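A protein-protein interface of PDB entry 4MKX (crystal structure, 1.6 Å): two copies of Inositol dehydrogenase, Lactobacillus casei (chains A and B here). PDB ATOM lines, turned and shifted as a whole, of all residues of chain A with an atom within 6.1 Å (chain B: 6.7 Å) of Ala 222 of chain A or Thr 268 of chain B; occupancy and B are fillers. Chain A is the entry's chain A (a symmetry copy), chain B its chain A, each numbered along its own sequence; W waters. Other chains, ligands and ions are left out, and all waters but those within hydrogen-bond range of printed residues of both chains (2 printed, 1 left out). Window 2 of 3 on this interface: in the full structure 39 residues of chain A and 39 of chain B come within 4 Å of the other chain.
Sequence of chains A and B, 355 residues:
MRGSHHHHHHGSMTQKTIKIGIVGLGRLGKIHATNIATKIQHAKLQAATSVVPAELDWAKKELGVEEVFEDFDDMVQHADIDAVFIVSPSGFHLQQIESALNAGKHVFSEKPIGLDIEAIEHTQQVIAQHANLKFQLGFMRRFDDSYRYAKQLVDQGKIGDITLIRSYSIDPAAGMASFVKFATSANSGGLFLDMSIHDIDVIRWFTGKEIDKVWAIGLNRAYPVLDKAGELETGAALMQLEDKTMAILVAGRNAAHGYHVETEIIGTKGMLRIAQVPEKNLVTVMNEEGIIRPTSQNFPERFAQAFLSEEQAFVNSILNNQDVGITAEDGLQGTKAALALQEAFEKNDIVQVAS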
ATOM      1  N   ASN A 220       7.538 -35.740 -14.385  1.00  0.00           N
ATOM      2  CA  ASN A 220       6.603 -35.843 -13.271  1.00  0.00           C
ATOM      3  C   ASN A 220       7.084 -35.107 -12.013  1.00  0.00           C
ATOM      4  O   ASN A 220       7.361 -35.728 -10.986  1.00  0.00           O
ATOM      5  CB  ASN A 220       6.327 -37.302 -12.972  1.00  0.00           C
ATOM      6  CG  ASN A 220       5.555 -37.968 -14.077  1.00  0.00           C
ATOM      7  OD1 ASN A 220       4.573 -37.411 -14.572  1.00  0.00           O
ATOM      8  ND2 ASN A 220       5.999 -39.149 -14.492  1.00  0.00           N
ATOM      9  N   ARG A 221       7.157 -33.781 -12.096  1.00  0.00           N
ATOM     10  CA  ARG A 221       7.766 -32.974 -11.039  1.00  0.00           C
ATOM     11  C   ARG A 221       6.875 -32.883  -9.808  1.00  0.00           C
ATOM     12  O   ARG A 221       7.307 -33.165  -8.691  1.00  0.00           O
ATOM     13  CB  ARG A 221       8.053 -31.561 -11.549  1.00  0.00           C
ATOM     14  CG  ARG A 221       8.983 -30.764 -10.645  1.00  0.00           C
ATOM     15  CD  ARG A 221      10.407 -30.956 -11.125  1.00  0.00           C
ATOM     16  NE  ARG A 221      10.690 -30.074 -12.247  1.00  0.00           N
ATOM     17  CZ  ARG A 221      11.793 -30.123 -12.986  1.00  0.00           C
ATOM     18  NH1 ARG A 221      12.734 -31.028 -12.744  1.00  0.00           N
ATOM     19  NH2 ARG A 221      11.938 -29.273 -13.988  1.00  0.00           N
ATOM     20  N   ALA A 222       5.626 -32.480 -10.023  1.00  0.00           N
ATOM     21  CA  ALA A 222       4.686 -32.279  -8.922  1.00  0.00           C
ATOM     22  C   ALA A 222       4.226 -33.601  -8.295  1.00  0.00           C
ATOM     23  O   ALA A 222       3.981 -33.672  -7.085  1.00  0.00           O
ATOM     24  CB  ALA A 222       3.490 -31.456  -9.391  1.00  0.00           C
ATOM     25  N   TYR A 223       4.090 -34.632  -9.128  1.00  0.00           N
ATOM     26  CA  TYR A 223       3.670 -35.956  -8.671  1.00  0.00           C
ATOM     27  C   TYR A 223       4.576 -37.056  -9.252  1.00  0.00           C
ATOM     28  O   TYR A 223       4.190 -37.737 -10.210  1.00  0.00           O
ATOM     29  CB  TYR A 223       2.208 -36.227  -9.067  1.00  0.00           C
ATOM     30  CG  TYR A 223       1.188 -35.235  -8.520  1.00  0.00           C
ATOM     31  CD1 TYR A 223       1.005 -33.988  -9.117  1.00  0.00           C
ATOM     32  CD2 TYR A 223       0.391 -35.557  -7.421  1.00  0.00           C
ATOM     33  CE1 TYR A 223       0.075 -33.078  -8.626  1.00  0.00           C
ATOM     34  CE2 TYR A 223      -0.550 -34.648  -6.919  1.00  0.00           C
ATOM     35  CZ  TYR A 223      -0.702 -33.415  -7.527  1.00  0.00           C
ATOM     36  OH  TYR A 223      -1.627 -32.506  -7.040  1.00  0.00           O
ATOM     37  N   PRO A 224       5.786 -37.230  -8.681  1.00  0.00           N
ATOM     38  CA  PRO A 224       6.737 -38.253  -9.147  1.00  0.00           C
ATOM     39  C   PRO A 224       6.259 -39.704  -9.061  1.00  0.00           C
ATOM     40  O   PRO A 224       6.919 -40.575  -9.632  1.00  0.00           O
ATOM     41  CB  PRO A 224       7.949 -38.043  -8.231  1.00  0.00           C
ATOM     42  CG  PRO A 224       7.917 -36.580  -7.929  1.00  0.00           C
ATOM     43  CD  PRO A 224       6.434 -36.275  -7.765  1.00  0.00           C
ATOM     44  N   GLU A 233       2.667 -36.226 -15.983  1.00  0.00           N
ATOM     45  CA  GLU A 233       1.854 -35.098 -15.551  1.00  0.00           C
ATOM     46  C   GLU A 233       1.960 -33.918 -16.518  1.00  0.00           C
ATOM     47  O   GLU A 233       0.996 -33.179 -16.699  1.00  0.00           O
ATOM     48  CB  GLU A 233       2.235 -34.665 -14.137  1.00  0.00           C
ATOM     49  CG  GLU A 233       3.568 -33.995 -14.054  1.00  0.00           C
ATOM     50  CD  GLU A 233       3.858 -33.454 -12.683  1.00  0.00           C
ATOM     51  OE1 GLU A 233       3.450 -34.110 -11.697  1.00  0.00           O
ATOM     52  OE2 GLU A 233       4.502 -32.387 -12.602  1.00  0.00           O
ATOM     53  N   ASN A 254      -2.027 -30.824 -14.682  1.00  0.00           N
ATOM     54  CA  ASN A 254      -1.841 -30.047 -13.460  1.00  0.00           C
ATOM     55  C   ASN A 254      -1.875 -28.522 -13.631  1.00  0.00           C
ATOM     56  O   ASN A 254      -0.978 -27.822 -13.162  1.00  0.00           O
ATOM     57  CB  ASN A 254      -0.522 -30.464 -12.794  1.00  0.00           C
ATOM     58  CG  ASN A 254      -0.442 -30.050 -11.335  1.00  0.00           C
ATOM     59  OD1 ASN A 254      -1.451 -30.031 -10.631  1.00  0.00           O
ATOM     60  ND2 ASN A 254       0.763 -29.713 -10.878  1.00  0.00           N
ATOM     61  N   ALA A 256      -3.066 -25.002 -12.569  1.00  0.00           N
ATOM     62  CA  ALA A 256      -3.627 -24.432 -11.352  1.00  0.00           C
ATOM     63  C   ALA A 256      -4.815 -23.509 -11.624  1.00  0.00           C
ATOM     64  O   ALA A 256      -5.687 -23.341 -10.763  1.00  0.00           O
ATOM     65  CB  ALA A 256      -2.549 -23.697 -10.565  1.00  0.00           C
ATOM     66  N   ILE B 159       5.235 -19.747  -7.818  1.00  0.00           N
ATOM     67  CA  ILE B 159       4.720 -20.696  -8.794  1.00  0.00           C
ATOM     68  C   ILE B 159       5.328 -22.076  -8.613  1.00  0.00           C
ATOM     69  O   ILE B 159       5.129 -22.958  -9.443  1.00  0.00           O
ATOM     70  CB  ILE B 159       4.882 -20.242 -10.262  1.00  0.00           C
ATOM     71  CG1 ILE B 159       6.354 -20.196 -10.649  1.00  0.00           C
ATOM     72  CG2 ILE B 159       4.183 -18.903 -10.507  1.00  0.00           C
ATOM     73  CD1 ILE B 159       6.560 -20.238 -12.139  1.00  0.00           C
ATOM     74  N   GLY B 160       6.061 -22.256  -7.517  1.00  0.00           N
ATOM     75  CA  GLY B 160       6.627 -23.560  -7.205  1.00  0.00           C
ATOM     76  C   GLY B 160       7.854 -23.809  -8.052  1.00  0.00           C
ATOM     77  O   GLY B 160       8.497 -22.863  -8.511  1.00  0.00           O
ATOM     78  N   ASP B 161       8.186 -25.076  -8.270  1.00  0.00           N
ATOM     79  CA  ASP B 161       9.322 -25.394  -9.125  1.00  0.00           C
ATOM     80  C   ASP B 161       8.887 -25.245 -10.579  1.00  0.00           C
ATOM     81  O   ASP B 161       7.725 -25.473 -10.921  1.00  0.00           O
ATOM     82  CB  ASP B 161       9.828 -26.812  -8.844  1.00  0.00           C
ATOM     83  CG  ASP B 161      11.068 -27.160  -9.654  1.00  0.00           C
ATOM     84  OD1 ASP B 161      11.875 -26.259  -9.975  1.00  0.00           O
ATOM     85  OD2 ASP B 161      11.238 -28.349  -9.973  1.00  0.00           O
ATOM     86  N   ILE B 162       9.827 -24.864 -11.435  1.00  0.00           N
ATOM     87  CA  ILE B 162       9.531 -24.629 -12.838  1.00  0.00           C
ATOM     88  C   ILE B 162       9.537 -25.930 -13.624  1.00  0.00           C
ATOM     89  O   ILE B 162      10.472 -26.711 -13.538  1.00  0.00           O
ATOM     90  CB  ILE B 162      10.561 -23.656 -13.425  1.00  0.00           C
ATOM     91  CG1 ILE B 162      10.400 -22.299 -12.744  1.00  0.00           C
ATOM     92  CG2 ILE B 162      10.401 -23.576 -14.945  1.00  0.00           C
ATOM     93  CD1 ILE B 162      11.477 -21.284 -13.112  1.00  0.00           C
ATOM     94  N   THR B 163       8.478 -26.185 -14.382  1.00  0.00           N
ATOM     95  CA  THR B 163       8.412 -27.409 -15.170  1.00  0.00           C
ATOM     96  C   THR B 163       8.659 -27.137 -16.656  1.00  0.00           C
ATOM     97  O   THR B 163       9.189 -27.972 -17.363  1.00  0.00           O
ATOM     98  CB  THR B 163       7.054 -28.078 -15.031  1.00  0.00           C
ATOM     99  OG1 THR B 163       6.089 -27.265 -15.692  1.00  0.00           O
ATOM    100  CG2 THR B 163       6.662 -28.219 -13.581  1.00  0.00           C
ATOM    101  N   ILE B 266       5.807 -22.102 -16.687  1.00  0.00           N
ATOM    102  CA  ILE B 266       4.823 -22.972 -16.057  1.00  0.00           C
ATOM    103  C   ILE B 266       5.468 -23.635 -14.849  1.00  0.00           C
ATOM    104  O   ILE B 266       6.542 -24.229 -14.962  1.00  0.00           O
ATOM    105  CB  ILE B 266       4.358 -24.062 -17.017  1.00  0.00           C
ATOM    106  CG1 ILE B 266       3.772 -23.418 -18.280  1.00  0.00           C
ATOM    107  CG2 ILE B 266       3.297 -24.916 -16.342  1.00  0.00           C
ATOM    108  CD1 ILE B 266       3.215 -24.414 -19.280  1.00  0.00           C
ATOM    109  N   GLY B 267       4.841 -23.488 -13.690  1.00  0.00           N
ATOM    110  CA  GLY B 267       5.376 -24.065 -12.468  1.00  0.00           C
ATOM    111  C   GLY B 267       4.393 -25.070 -11.888  1.00  0.00           C
ATOM    112  O   GLY B 267       3.318 -25.310 -12.445  1.00  0.00           O
ATOM    113  N   THR B 268       4.755 -25.659 -10.760  1.00  0.00           N
ATOM    114  CA  THR B 268       3.898 -26.666 -10.150  1.00  0.00           C
ATOM    115  C   THR B 268       2.701 -26.019  -9.466  1.00  0.00           C
ATOM    116  O   THR B 268       1.700 -26.688  -9.228  1.00  0.00           O
ATOM    117  CB  THR B 268       4.682 -27.530  -9.143  1.00  0.00           C
ATOM    118  OG1 THR B 268       5.311 -26.683  -8.176  1.00  0.00           O
ATOM    119  CG2 THR B 268       5.734 -28.360  -9.863  1.00  0.00           C
ATOM    120  N   LYS B 269       2.781 -24.722  -9.168  1.00  0.00           N
ATOM    121  CA  LYS B 269       1.727 -24.047  -8.414  1.00  0.00           C
ATOM    122  C   LYS B 269       1.075 -22.912  -9.190  1.00  0.00           C
ATOM    123  O   LYS B 269       0.184 -22.228  -8.673  1.00  0.00           O
ATOM    124  CB  LYS B 269       2.280 -23.474  -7.112  1.00  0.00           C
ATOM    125  CG  LYS B 269       3.082 -24.464  -6.290  1.00  0.00           C
ATOM    126  CD  LYS B 269       3.210 -23.988  -4.860  1.00  0.00           C
ATOM    127  CE  LYS B 269       3.616 -22.532  -4.813  1.00  0.00           C
ATOM    128  NZ  LYS B 269       3.391 -21.910  -3.476  1.00  0.00           N
ATOM    129  N   GLY B 270       1.529 -22.699 -10.420  1.00  0.00           N
ATOM    130  CA  GLY B 270       1.039 -21.564 -11.176  1.00  0.00           C
ATOM    131  C   GLY B 270       1.767 -21.365 -12.485  1.00  0.00           C
ATOM    132  O   GLY B 270       2.610 -22.167 -12.881  1.00  0.00           O
HETATM  133  O   HOH W   1      -1.151 -27.185  -9.595  1.00  0.00           O
HETATM  134  O   HOH W   2       1.294 -29.118  -7.523  1.00  0.00           O
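The guanidinium group of Arg 221 of chain A is in salt-bridge range of the side-chain carboxylate of Asp 161 of chain B (2.9 Å). NH2 of Arg 221 of chain A lies within hydrogen-bond range of O of Ile 162 of chain B (3.0 Å).
The backbone carbonyl oxygen (O) of Ile 159 of chain B lies within hydrogen-bond range of the backbone NH (N) of Thr 268 of chain B (3.0 Å). The backbone carbonyl oxygen (O) of Ile 159 of chain B lies within hydrogen-bond range of the backbone NH (N) of Lys 269 of chain B. The backbone NH (N) of Thr 268 of chain B is in hydrogen-bond range of the backbone carbonyl oxygen (O) of Asp 161 of chain B (3.0 Å). The backbone NH of Arg 221 of chain A is in hydrogen-bond range of the side-chain carboxylate of Glu 233 of chain A (3.0 Å). OE2 of Glu 233 of chain A lies within hydrogen-bond range of N of Ala 222 of chain A (2.8 Å).
Among the printed residues, merely in contact across the chains: Asn 254 of chain A with Thr 268 of chain B (3.6 Å), Ala 256 of chain A with Lys 269 of chain B (3.6 Å) and Ala 222 of chain A with Thr 268 of chain B (3.9 Å).
Printed residues of chain B within 4 Å of Arg 221 of chain A: Asp 161 (2.9 Å) and Ile 162 (3.0 Å). Of the printed residues of chain B, Ala 222 of chain A touches Thr 268. Glu 233 of chain A touches none of the printed residues of chain B. Of the printed residues of chain B, Ala 256 of chain A touches Lys 269. Of the printed residues of chain A, Asp 161 of chain B touches Arg 221. Thr 268 of chain B touches just these residues of chain A: Ala 222 and Asn 254. The nearest residue of chain B that does not touch Ala 222 of chain A is Thr 163 of chain B (5.6 Å). The nearest residue of chain A that does not touch Thr 268 of chain B is Arg 221 of chain A (4.1 Å). The nearest printed residue of chain A that does not touch Lys 269 of chain B is Asn 254 of chain A (5.6 Å).
Of the 10 printed residues of chain B, 4 touch a printed residue of chain A. Along chain B the printed residues that touch a printed residue of chain A span positions 161 to 269. Of the 8 printed residues of chain A, 4 touch a printed residue of chain B. Printed residues of chain A that touch a printed residue of chain B: Arg 221, Ala 222, Asn 254 and Ala 256. Hydrophobic or aromatic side chains of chain A that line the printed part of chain B: Ala 222 and Ala 256. Among the printed residues, Asp or Glu carboxylates within 4 Å of a Lys or Arg side-chain nitrogen of the other chain: Arg 221 of chain A with Asp 161 of chain B (2.9 Å).
No position is printed for both chains. Of the 5 pairs that touch across the chains among the printed residues, none has its exchanged pair printed and touching as well.
Water W1 bridges the backbone carbonyl oxygen of Thr 268 of chain B and the side-chain amide oxygen of Asn 254 of chain A. Water W2 lies within hydrogen-bond range of O of Thr 268 of chain B (3.0 Å) and ND2 of Asn 254 of chain A (3.4 Å).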
